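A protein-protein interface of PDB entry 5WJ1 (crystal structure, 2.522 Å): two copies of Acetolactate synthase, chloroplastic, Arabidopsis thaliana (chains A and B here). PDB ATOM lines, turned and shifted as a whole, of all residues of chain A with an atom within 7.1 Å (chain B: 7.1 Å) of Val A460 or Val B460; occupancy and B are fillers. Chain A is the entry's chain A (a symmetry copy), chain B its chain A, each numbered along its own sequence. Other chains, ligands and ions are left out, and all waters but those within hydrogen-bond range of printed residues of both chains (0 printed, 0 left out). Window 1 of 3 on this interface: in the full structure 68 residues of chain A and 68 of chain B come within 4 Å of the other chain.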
ATOM      1  N   ARG A  57      11.668  26.419  13.382  1.00  0.00           N
ATOM      2  CA  ARG A  57      11.875  26.123  14.792  1.00  0.00           C
ATOM      3  C   ARG A  57      13.350  25.841  15.065  1.00  0.00           C
ATOM      4  O   ARG A  57      13.747  25.550  16.193  1.00  0.00           O
ATOM      5  CB  ARG A  57      11.002  24.948  15.223  1.00  0.00           C
ATOM      6  CG  ARG A  57       9.713  25.369  15.911  1.00  0.00           C
ATOM      7  CD  ARG A  57       8.910  26.318  15.039  1.00  0.00           C
ATOM      8  NE  ARG A  57       7.670  26.746  15.681  1.00  0.00           N
ATOM      9  CZ  ARG A  57       6.811  27.603  15.140  1.00  0.00           C
ATOM     10  NH1 ARG A  57       7.059  28.128  13.946  1.00  0.00           N
ATOM     11  NH2 ARG A  57       5.706  27.938  15.792  1.00  0.00           N
ATOM     12  N   GLY A 429      18.191  15.232   7.473  1.00  0.00           N
ATOM     13  CA  GLY A 429      17.383  16.299   8.043  1.00  0.00           C
ATOM     14  C   GLY A 429      16.938  17.320   7.011  1.00  0.00           C
ATOM     15  O   GLY A 429      16.296  18.314   7.346  1.00  0.00           O
ATOM     16  N   LEU A 432      12.246  17.283   5.318  1.00  0.00           N
ATOM     17  CA  LEU A 432      11.079  17.985   5.844  1.00  0.00           C
ATOM     18  C   LEU A 432      11.165  19.512   5.659  1.00  0.00           C
ATOM     19  O   LEU A 432      10.212  20.119   5.167  1.00  0.00           O
ATOM     20  CB  LEU A 432      10.870  17.630   7.323  1.00  0.00           C
ATOM     21  CG  LEU A 432       9.519  18.010   7.925  1.00  0.00           C
ATOM     22  CD1 LEU A 432       8.413  17.195   7.271  1.00  0.00           C
ATOM     23  CD2 LEU A 432       9.527  17.812   9.435  1.00  0.00           C
ATOM     24  N   PRO A 433      12.297  20.142   6.040  1.00  0.00           N
ATOM     25  CA  PRO A 433      12.369  21.590   5.795  1.00  0.00           C
ATOM     26  C   PRO A 433      12.330  21.959   4.311  1.00  0.00           C
ATOM     27  O   PRO A 433      11.726  22.970   3.957  1.00  0.00           O
ATOM     28  CB  PRO A 433      13.719  21.987   6.404  1.00  0.00           C
ATOM     29  CG  PRO A 433      14.065  20.899   7.338  1.00  0.00           C
ATOM     30  CD  PRO A 433      13.491  19.656   6.756  1.00  0.00           C
ATOM     31  N   SER A 455      16.665  10.328   9.393  1.00  0.00           N
ATOM     32  CA  SER A 455      16.668  11.655   8.789  1.00  0.00           C
ATOM     33  C   SER A 455      15.505  12.518   9.271  1.00  0.00           C
ATOM     34  O   SER A 455      15.670  13.714   9.517  1.00  0.00           O
ATOM     35  CB  SER A 455      16.614  11.542   7.262  1.00  0.00           C
ATOM     36  OG  SER A 455      17.755  10.879   6.744  1.00  0.00           O
ATOM     37  N   PHE A 456      14.328  11.908   9.390  1.00  0.00           N
ATOM     38  CA  PHE A 456      13.111  12.631   9.749  1.00  0.00           C
ATOM     39  C   PHE A 456      13.178  13.230  11.147  1.00  0.00           C
ATOM     40  O   PHE A 456      12.731  14.356  11.367  1.00  0.00           O
ATOM     41  CB  PHE A 456      11.891  11.709   9.646  1.00  0.00           C
ATOM     42  CG  PHE A 456      10.604  12.351  10.079  1.00  0.00           C
ATOM     43  CD1 PHE A 456       9.930  13.221   9.235  1.00  0.00           C
ATOM     44  CD2 PHE A 456      10.063  12.082  11.327  1.00  0.00           C
ATOM     45  CE1 PHE A 456       8.740  13.814   9.629  1.00  0.00           C
ATOM     46  CE2 PHE A 456       8.875  12.671  11.729  1.00  0.00           C
ATOM     47  CZ  PHE A 456       8.213  13.538  10.879  1.00  0.00           C
ATOM     48  N   ILE A 457      13.728  12.477  12.093  1.00  0.00           N
ATOM     49  CA  ILE A 457      13.736  12.916  13.482  1.00  0.00           C
ATOM     50  C   ILE A 457      14.747  14.034  13.709  1.00  0.00           C
ATOM     51  O   ILE A 457      14.639  14.787  14.677  1.00  0.00           O
ATOM     52  CB  ILE A 457      14.036  11.745  14.450  1.00  0.00           C
ATOM     53  CG1 ILE A 457      13.511  12.069  15.853  1.00  0.00           C
ATOM     54  CG2 ILE A 457      15.523  11.408  14.466  1.00  0.00           C
ATOM     55  CD1 ILE A 457      13.760  10.981  16.872  1.00  0.00           C
ATOM     56  N   MET A 458      15.715  14.157  12.806  1.00  0.00           N
ATOM     57  CA  MET A 458      16.764  15.162  12.958  1.00  0.00           C
ATOM     58  C   MET A 458      16.220  16.583  12.963  1.00  0.00           C
ATOM     59  O   MET A 458      16.717  17.435  13.693  1.00  0.00           O
ATOM     60  CB  MET A 458      17.808  15.020  11.857  1.00  0.00           C
ATOM     61  CG  MET A 458      18.935  14.080  12.216  1.00  0.00           C
ATOM     62  SD  MET A 458      20.404  14.391  11.233  1.00  0.00           S
ATOM     63  CE  MET A 458      21.525  13.166  11.907  1.00  0.00           C
ATOM     64  N   ASN A 459      15.205  16.840  12.146  1.00  0.00           N
ATOM     65  CA  ASN A 459      14.575  18.153  12.124  1.00  0.00           C
ATOM     66  C   ASN A 459      13.076  18.032  12.310  1.00  0.00           C
ATOM     67  O   ASN A 459      12.295  18.751  11.684  1.00  0.00           O
ATOM     68  CB  ASN A 459      14.899  18.884  10.824  1.00  0.00           C
ATOM     69  CG  ASN A 459      16.250  19.566  10.872  1.00  0.00           C
ATOM     70  OD1 ASN A 459      16.590  20.215  11.863  1.00  0.00           O
ATOM     71  ND2 ASN A 459      17.036  19.408   9.814  1.00  0.00           N
ATOM     72  N   VAL A 460      12.687  17.122  13.194  1.00  0.00           N
ATOM     73  CA  VAL A 460      11.287  16.827  13.449  1.00  0.00           C
ATOM     74  C   VAL A 460      10.544  18.055  13.983  1.00  0.00           C
ATOM     75  O   VAL A 460       9.324  18.147  13.869  1.00  0.00           O
ATOM     76  CB  VAL A 460      11.149  15.650  14.440  1.00  0.00           C
ATOM     77  CG1 VAL A 460      11.633  16.059  15.826  1.00  0.00           C
ATOM     78  CG2 VAL A 460       9.716  15.137  14.485  1.00  0.00           C
ATOM     79  N   GLN A 461      11.286  19.013  14.535  1.00  0.00           N
ATOM     80  CA  GLN A 461      10.678  20.213  15.103  1.00  0.00           C
ATOM     81  C   GLN A 461       9.982  21.073  14.049  1.00  0.00           C
ATOM     82  O   GLN A 461       9.165  21.930  14.383  1.00  0.00           O
ATOM     83  CB  GLN A 461      11.724  21.055  15.840  1.00  0.00           C
ATOM     84  CG  GLN A 461      12.661  21.846  14.940  1.00  0.00           C
ATOM     85  CD  GLN A 461      13.733  20.984  14.310  1.00  0.00           C
ATOM     86  OE1 GLN A 461      14.009  19.877  14.775  1.00  0.00           O
ATOM     87  NE2 GLN A 461      14.344  21.486  13.244  1.00  0.00           N
ATOM     88  N   GLU A 462      10.289  20.843  12.778  1.00  0.00           N
ATOM     89  CA  GLU A 462       9.691  21.646  11.718  1.00  0.00           C
ATOM     90  C   GLU A 462       8.250  21.221  11.418  1.00  0.00           C
ATOM     91  O   GLU A 462       7.567  21.850  10.608  1.00  0.00           O
ATOM     92  CB  GLU A 462      10.544  21.579  10.449  1.00  0.00           C
ATOM     93  CG  GLU A 462      11.989  22.053  10.638  1.00  0.00           C
ATOM     94  CD  GLU A 462      12.102  23.408  11.333  1.00  0.00           C
ATOM     95  OE1 GLU A 462      11.253  24.293  11.089  1.00  0.00           O
ATOM     96  OE2 GLU A 462      13.051  23.586  12.126  1.00  0.00           O
ATOM     97  N   LEU A 463       7.790  20.161  12.076  1.00  0.00           N
ATOM     98  CA  LEU A 463       6.378  19.793  12.035  1.00  0.00           C
ATOM     99  C   LEU A 463       5.520  20.932  12.580  1.00  0.00           C
ATOM    100  O   LEU A 463       4.410  21.169  12.105  1.00  0.00           O
ATOM    101  CB  LEU A 463       6.119  18.515  12.835  1.00  0.00           C
ATOM    102  CG  LEU A 463       6.647  17.202  12.258  1.00  0.00           C
ATOM    103  CD1 LEU A 463       6.320  16.049  13.193  1.00  0.00           C
ATOM    104  CD2 LEU A 463       6.064  16.956  10.876  1.00  0.00           C
ATOM    105  N   ALA A 464       6.046  21.629  13.583  1.00  0.00           N
ATOM    106  CA  ALA A 464       5.366  22.775  14.168  1.00  0.00           C
ATOM    107  C   ALA A 464       5.228  23.894  13.144  1.00  0.00           C
ATOM    108  O   ALA A 464       4.193  24.557  13.067  1.00  0.00           O
ATOM    109  CB  ALA A 464       6.115  23.266  15.399  1.00  0.00           C
ATOM    110  N   THR A 465       6.280  24.094  12.359  1.00  0.00           N
ATOM    111  CA  THR A 465       6.273  25.092  11.298  1.00  0.00           C
ATOM    112  C   THR A 465       5.206  24.763  10.260  1.00  0.00           C
ATOM    113  O   THR A 465       4.487  25.644   9.793  1.00  0.00           O
ATOM    114  CB  THR A 465       7.642  25.181  10.604  1.00  0.00           C
ATOM    115  OG1 THR A 465       8.672  25.329  11.588  1.00  0.00           O
ATOM    116  CG2 THR A 465       7.685  26.365   9.647  1.00  0.00           C
ATOM    117  N   MET A 516       6.359   7.875  15.660  1.00  0.00           N
ATOM    118  CA  MET A 516       6.342   9.089  14.853  1.00  0.00           C
ATOM    119  C   MET A 516       4.939   9.680  14.726  1.00  0.00           C
ATOM    120  O   MET A 516       4.783  10.872  14.455  1.00  0.00           O
ATOM    121  CB  MET A 516       6.924   8.805  13.466  1.00  0.00           C
ATOM    122  CG  MET A 516       8.355   8.282  13.492  1.00  0.00           C
ATOM    123  SD  MET A 516       9.501   9.427  14.287  1.00  0.00           S
ATOM    124  CE  MET A 516      11.074   8.685  13.854  1.00  0.00           C
ATOM    125  N   PHE A 519       4.616  12.322  17.291  1.00  0.00           N
ATOM    126  CA  PHE A 519       5.317  13.549  16.915  1.00  0.00           C
ATOM    127  C   PHE A 519       4.374  14.432  16.111  1.00  0.00           C
ATOM    128  O   PHE A 519       4.289  15.638  16.336  1.00  0.00           O
ATOM    129  CB  PHE A 519       6.580  13.251  16.103  1.00  0.00           C
ATOM    130  CG  PHE A 519       7.764  12.856  16.940  1.00  0.00           C
ATOM    131  CD1 PHE A 519       8.331  13.753  17.824  1.00  0.00           C
ATOM    132  CD2 PHE A 519       8.321  11.595  16.828  1.00  0.00           C
ATOM    133  CE1 PHE A 519       9.421  13.400  18.593  1.00  0.00           C
ATOM    134  CE2 PHE A 519       9.416  11.234  17.595  1.00  0.00           C
ATOM    135  CZ  PHE A 519       9.964  12.136  18.478  1.00  0.00           C
ATOM    136  N   ALA A 520       3.657  13.811  15.180  1.00  0.00           N
ATOM    137  CA  ALA A 520       2.693  14.520  14.349  1.00  0.00           C
ATOM    138  C   ALA A 520       1.517  15.018  15.184  1.00  0.00           C
ATOM    139  O   ALA A 520       1.070  16.155  15.025  1.00  0.00           O
ATOM    140  CB  ALA A 520       2.205  13.621  13.223  1.00  0.00           C
ATOM    141  N   CYS A 523       1.943  18.168  17.046  1.00  0.00           N
ATOM    142  CA  CYS A 523       1.836  19.383  16.251  1.00  0.00           C
ATOM    143  C   CYS A 523       0.521  19.440  15.481  1.00  0.00           C
ATOM    144  O   CYS A 523       0.412  20.143  14.481  1.00  0.00           O
ATOM    145  CB  CYS A 523       3.017  19.493  15.287  1.00  0.00           C
ATOM    146  SG  CYS A 523       4.629  19.528  16.106  1.00  0.00           S
ATOM    147  N   ARG B  57      20.687  11.677  18.304  1.00  0.00           N
ATOM    148  CA  ARG B  57      19.827  11.651  17.130  1.00  0.00           C
ATOM    149  C   ARG B  57      20.156  12.819  16.205  1.00  0.00           C
ATOM    150  O   ARG B  57      19.536  13.000  15.158  1.00  0.00           O
ATOM    151  CB  ARG B  57      18.358  11.677  17.545  1.00  0.00           C
ATOM    152  CG  ARG B  57      17.706  10.303  17.558  1.00  0.00           C
ATOM    153  CD  ARG B  57      18.478   9.338  18.442  1.00  0.00           C
ATOM    154  NE  ARG B  57      17.879   8.007  18.465  1.00  0.00           N
ATOM    155  CZ  ARG B  57      18.383   6.976  19.134  1.00  0.00           C
ATOM    156  NH1 ARG B  57      19.501   7.123  19.834  1.00  0.00           N
ATOM    157  NH2 ARG B  57      17.774   5.799  19.102  1.00  0.00           N
ATOM    158  N   GLY B 429      18.777  25.129  22.546  1.00  0.00           N
ATOM    159  CA  GLY B 429      18.872  23.711  22.234  1.00  0.00           C
ATOM    160  C   GLY B 429      19.943  22.998  23.040  1.00  0.00           C
ATOM    161  O   GLY B 429      20.184  21.807  22.849  1.00  0.00           O
ATOM    162  N   LEU B 432      18.659  20.100  26.892  1.00  0.00           N
ATOM    163  CA  LEU B 432      18.350  18.674  26.899  1.00  0.00           C
ATOM    164  C   LEU B 432      19.580  17.792  26.609  1.00  0.00           C
ATOM    165  O   LEU B 432      19.838  16.844  27.352  1.00  0.00           O
ATOM    166  CB  LEU B 432      17.221  18.372  25.904  1.00  0.00           C
ATOM    167  CG  LEU B 432      16.557  17.002  26.030  1.00  0.00           C
ATOM    168  CD1 LEU B 432      15.811  16.907  27.353  1.00  0.00           C
ATOM    169  CD2 LEU B 432      15.623  16.745  24.855  1.00  0.00           C
ATOM    170  N   PRO B 433      20.349  18.096  25.541  1.00  0.00           N
ATOM    171  CA  PRO B 433      21.547  17.272  25.326  1.00  0.00           C
ATOM    172  C   PRO B 433      22.576  17.389  26.453  1.00  0.00           C
ATOM    173  O   PRO B 433      23.210  16.393  26.797  1.00  0.00           O
ATOM    174  CB  PRO B 433      22.130  17.824  24.020  1.00  0.00           C
ATOM    175  CG  PRO B 433      21.017  18.535  23.362  1.00  0.00           C
ATOM    176  CD  PRO B 433      20.171  19.081  24.458  1.00  0.00           C
ATOM    177  N   SER B 455      13.556  26.719  23.064  1.00  0.00           N
ATOM    178  CA  SER B 455      14.825  26.017  23.209  1.00  0.00           C
ATOM    179  C   SER B 455      14.657  24.500  23.208  1.00  0.00           C
ATOM    180  O   SER B 455      15.460  23.780  22.611  1.00  0.00           O
ATOM    181  CB  SER B 455      15.524  26.447  24.502  1.00  0.00           C
ATOM    182  OG  SER B 455      15.845  27.828  24.492  1.00  0.00           O
ATOM    183  N   PHE B 456      13.618  24.023  23.889  1.00  0.00           N
ATOM    184  CA  PHE B 456      13.390  22.590  24.053  1.00  0.00           C
ATOM    185  C   PHE B 456      13.113  21.886  22.730  1.00  0.00           C
ATOM    186  O   PHE B 456      13.599  20.780  22.497  1.00  0.00           O
ATOM    187  CB  PHE B 456      12.225  22.342  25.018  1.00  0.00           C
ATOM    188  CG  PHE B 456      11.868  20.890  25.179  1.00  0.00           C
ATOM    189  CD1 PHE B 456      12.626  20.061  25.992  1.00  0.00           C
ATOM    190  CD2 PHE B 456      10.769  20.355  24.523  1.00  0.00           C
ATOM    191  CE1 PHE B 456      12.298  18.724  26.146  1.00  0.00           C
ATOM    192  CE2 PHE B 456      10.436  19.019  24.671  1.00  0.00           C
ATOM    193  CZ  PHE B 456      11.201  18.202  25.484  1.00  0.00           C
ATOM    194  N   ILE B 457      12.327  22.524  21.870  1.00  0.00           N
ATOM    195  CA  ILE B 457      11.913  21.886  20.627  1.00  0.00           C
ATOM    196  C   ILE B 457      13.057  21.826  19.622  1.00  0.00           C
ATOM    197  O   ILE B 457      13.036  21.011  18.700  1.00  0.00           O
ATOM    198  CB  ILE B 457      10.702  22.609  19.989  1.00  0.00           C
ATOM    199  CG1 ILE B 457       9.954  21.661  19.046  1.00  0.00           C
ATOM    200  CG2 ILE B 457      11.133  23.889  19.279  1.00  0.00           C
ATOM    201  CD1 ILE B 457       8.753  22.281  18.371  1.00  0.00           C
ATOM    202  N   MET B 458      14.065  22.673  19.811  1.00  0.00           N
ATOM    203  CA  MET B 458      15.184  22.733  18.876  1.00  0.00           C
ATOM    204  C   MET B 458      15.950  21.421  18.790  1.00  0.00           C
ATOM    205  O   MET B 458      16.403  21.036  17.716  1.00  0.00           O
ATOM    206  CB  MET B 458      16.141  23.859  19.253  1.00  0.00           C
ATOM    207  CG  MET B 458      15.794  25.182  18.612  1.00  0.00           C
ATOM    208  SD  MET B 458      17.208  26.286  18.553  1.00  0.00           S
ATOM    209  CE  MET B 458      16.489  27.708  17.734  1.00  0.00           C
ATOM    210  N   ASN B 459      16.099  20.740  19.920  1.00  0.00           N
ATOM    211  CA  ASN B 459      16.763  19.443  19.930  1.00  0.00           C
ATOM    212  C   ASN B 459      15.892  18.399  20.601  1.00  0.00           C
ATOM    213  O   ASN B 459      16.379  17.536  21.333  1.00  0.00           O
ATOM    214  CB  ASN B 459      18.120  19.537  20.622  1.00  0.00           C
ATOM    215  CG  ASN B 459      19.200  20.050  19.695  1.00  0.00           C
ATOM    216  OD1 ASN B 459      19.299  19.616  18.546  1.00  0.00           O
ATOM    217  ND2 ASN B 459      20.006  20.989  20.178  1.00  0.00           N
ATOM    218  N   VAL B 460      14.596  18.483  20.325  1.00  0.00           N
ATOM    219  CA  VAL B 460      13.609  17.606  20.933  1.00  0.00           C
ATOM    220  C   VAL B 460      13.867  16.139  20.573  1.00  0.00           C
ATOM    221  O   VAL B 460      13.433  15.235  21.285  1.00  0.00           O
ATOM    222  CB  VAL B 460      12.181  18.013  20.508  1.00  0.00           C
ATOM    223  CG1 VAL B 460      11.965  17.736  19.025  1.00  0.00           C
ATOM    224  CG2 VAL B 460      11.134  17.309  21.359  1.00  0.00           C
ATOM    225  N   GLN B 461      14.602  15.906  19.488  1.00  0.00           N
ATOM    226  CA  GLN B 461      14.883  14.546  19.038  1.00  0.00           C
ATOM    227  C   GLN B 461      15.736  13.762  20.036  1.00  0.00           C
ATOM    228  O   GLN B 461      15.799  12.536  19.974  1.00  0.00           O
ATOM    229  CB  GLN B 461      15.576  14.558  17.673  1.00  0.00           C
ATOM    230  CG  GLN B 461      17.047  14.949  17.702  1.00  0.00           C
ATOM    231  CD  GLN B 461      17.252  16.439  17.871  1.00  0.00           C
ATOM    232  OE1 GLN B 461      16.341  17.234  17.635  1.00  0.00           O
ATOM    233  NE2 GLN B 461      18.454  16.826  18.282  1.00  0.00           N
ATOM    234  N   GLU B 462      16.381  14.461  20.962  1.00  0.00           N
ATOM    235  CA  GLU B 462      17.241  13.786  21.928  1.00  0.00           C
ATOM    236  C   GLU B 462      16.434  13.107  23.040  1.00  0.00           C
ATOM    237  O   GLU B 462      16.999  12.420  23.893  1.00  0.00           O
ATOM    238  CB  GLU B 462      18.252  14.768  22.523  1.00  0.00           C
ATOM    239  CG  GLU B 462      19.153  15.447  21.487  1.00  0.00           C
ATOM    240  CD  GLU B 462      19.809  14.470  20.514  1.00  0.00           C
ATOM    241  OE1 GLU B 462      20.182  13.352  20.929  1.00  0.00           O
ATOM    242  OE2 GLU B 462      19.953  14.828  19.325  1.00  0.00           O
ATOM    243  N   LEU B 463      15.117  13.295  23.024  1.00  0.00           N
ATOM    244  CA  LEU B 463      14.230  12.534  23.897  1.00  0.00           C
ATOM    245  C   LEU B 463      14.364  11.039  23.613  1.00  0.00           C
ATOM    246  O   LEU B 463      14.277  10.214  24.521  1.00  0.00           O
ATOM    247  CB  LEU B 463      12.775  12.970  23.716  1.00  0.00           C
ATOM    248  CG  LEU B 463      12.380  14.348  24.245  1.00  0.00           C
ATOM    249  CD1 LEU B 463      10.912  14.620  23.959  1.00  0.00           C
ATOM    250  CD2 LEU B 463      12.666  14.448  25.735  1.00  0.00           C
ATOM    251  N   ALA B 464      14.576  10.706  22.343  1.00  0.00           N
ATOM    252  CA  ALA B 464      14.777   9.323  21.931  1.00  0.00           C
ATOM    253  C   ALA B 464      16.055   8.764  22.543  1.00  0.00           C
ATOM    254  O   ALA B 464      16.096   7.613  22.980  1.00  0.00           O
ATOM    255  CB  ALA B 464      14.823   9.223  20.413  1.00  0.00           C
ATOM    256  N   THR B 465      17.094   9.591  22.573  1.00  0.00           N
ATOM    257  CA  THR B 465      18.364   9.213  23.177  1.00  0.00           C
ATOM    258  C   THR B 465      18.186   8.930  24.665  1.00  0.00           C
ATOM    259  O   THR B 465      18.734   7.966  25.194  1.00  0.00           O
ATOM    260  CB  THR B 465      19.421  10.315  22.995  1.00  0.00           C
ATOM    261  OG1 THR B 465      19.480  10.701  21.617  1.00  0.00           O
ATOM    262  CG2 THR B 465      20.791   9.826  23.441  1.00  0.00           C
ATOM    263  N   MET B 516       3.778  19.310  24.055  1.00  0.00           N
ATOM    264  CA  MET B 516       5.065  18.719  24.403  1.00  0.00           C
ATOM    265  C   MET B 516       4.912  17.364  25.093  1.00  0.00           C
ATOM    266  O   MET B 516       5.836  16.550  25.086  1.00  0.00           O
ATOM    267  CB  MET B 516       5.859  19.679  25.293  1.00  0.00           C
ATOM    268  CG  MET B 516       6.125  21.035  24.654  1.00  0.00           C
ATOM    269  SD  MET B 516       7.051  20.908  23.110  1.00  0.00           S
ATOM    270  CE  MET B 516       7.469  22.627  22.824  1.00  0.00           C
ATOM    271  N   PHE B 519       5.305  14.756  22.502  1.00  0.00           N
ATOM    272  CA  PHE B 519       6.701  14.560  22.121  1.00  0.00           C
ATOM    273  C   PHE B 519       7.325  13.520  23.040  1.00  0.00           C
ATOM    274  O   PHE B 519       8.032  12.619  22.590  1.00  0.00           O
ATOM    275  CB  PHE B 519       7.495  15.868  22.189  1.00  0.00           C
ATOM    276  CG  PHE B 519       7.313  16.755  20.990  1.00  0.00           C
ATOM    277  CD1 PHE B 519       7.750  16.349  19.744  1.00  0.00           C
ATOM    278  CD2 PHE B 519       6.725  18.001  21.114  1.00  0.00           C
ATOM    279  CE1 PHE B 519       7.590  17.161  18.638  1.00  0.00           C
ATOM    280  CE2 PHE B 519       6.563  18.820  20.009  1.00  0.00           C
ATOM    281  CZ  PHE B 519       6.995  18.398  18.772  1.00  0.00           C
ATOM    282  N   ALA B 520       7.044  13.650  24.332  1.00  0.00           N
ATOM    283  CA  ALA B 520       7.547  12.716  25.329  1.00  0.00           C
ATOM    284  C   ALA B 520       6.925  11.334  25.144  1.00  0.00           C
ATOM    285  O   ALA B 520       7.618  10.318  25.214  1.00  0.00           O
ATOM    286  CB  ALA B 520       7.274  13.239  26.731  1.00  0.00           C
ATOM    287  N   CYS B 523       8.395   9.115  22.597  1.00  0.00           N
ATOM    288  CA  CYS B 523       9.635   8.456  22.983  1.00  0.00           C
ATOM    289  C   CYS B 523       9.478   7.677  24.284  1.00  0.00           C
ATOM    290  O   CYS B 523      10.460   7.402  24.969  1.00  0.00           O
ATOM    291  CB  CYS B 523      10.762   9.481  23.112  1.00  0.00           C
ATOM    292  SG  CYS B 523      11.093  10.400  21.591  1.00  0.00           S
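Of the printed residues of chain B, Val A460 touches Val B460.
Of chain A, only Val A460 comes within 4 Å of Val B460.
Printed residues of chain A within 4 Å of Ile B457: Arg A57 and Gln A461.
Of the printed residues of chain B, Phe A519 touches Phe B519 and Cys B523.
Pro B433 touches none of the printed residues of chain A.
The nearest residue of chain A that does not touch Val B460 is Gln A461 (4.6 Å).
The nearest printed residue of chain A that does not touch Met B458 is Met A458 (5.4 Å).
Ile B457 touches Arg A57.
Ile A457 touches Arg B57 (CG2 to CG, 3.9 Å).
O of Arg B57 touches CG of Met A458 (3.2 Å).
OE1 of Gln B461 touches O of Met A458, at 3.96 Å.
Val B460 touches Val A460 (CG1 to CG1, 3.6 Å).
O of Ile B457 touches CB of Gln A461, at 3.1 Å.
OE1 of Gln A461 touches O of Met B458, 3.97 Å away.
CD1 of Phe A519 touches CD1 of Phe B519 (3.3 Å).
Phe A519 touches Cys B523.
SG of Cys A523 touches CZ of Phe B519, at 3.7 Å.
N of Arg B57 lies within hydrogen-bond range of OE1 of Glu B462.
The side-chain amide oxygen (OD1) of Asn B459 lies within hydrogen-bond range of the side-chain amide nitrogen (NE2) of Gln B461 (2.9 Å).
The side-chain carboxylate of Glu B462 sits at hydrogen-bond distance from the side-chain amide nitrogen of Gln B461 (2.7 Å).
N of Ala B464 is in hydrogen-bond range of SG of Cys B523 (3.6 Å).
The side-chain carboxylate (OE1) of Glu A462 is in hydrogen-bond range of the backbone NH (N) of Arg A57 (3.2 Å).
N of Ala A464 lies within hydrogen-bond range of SG of Cys A523 (3.6 Å).
Of the 19 printed residues of chain A, 7 touch a printed residue of chain B.
Hydrophobic or aromatic side chains of chain A that line the printed part of chain B: Ile A457, Met A458, Val A460 and Phe A519.
Along chain A the printed residues that touch a printed residue of chain B span positions 57 to 523.
Among the printed residues, 12 pairs touch across the chains.
Arg A57 touches Ile B457, and with the chains exchanged Ile A457 touches Arg B57.
Arg A57 touches Met B458, and with the chains exchanged Met A458 touches Arg B57.
Ile A457 touches Gln B461, and with the chains exchanged Gln A461 touches Ile B457.
Phe A519 touches Cys B523, and with the chains exchanged Cys A523 touches Phe B519.
19 positions are printed for both chains.
Of the 12 pairs that touch across the chains among the printed residues, 12 have their exchanged pair printed and touching as well.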
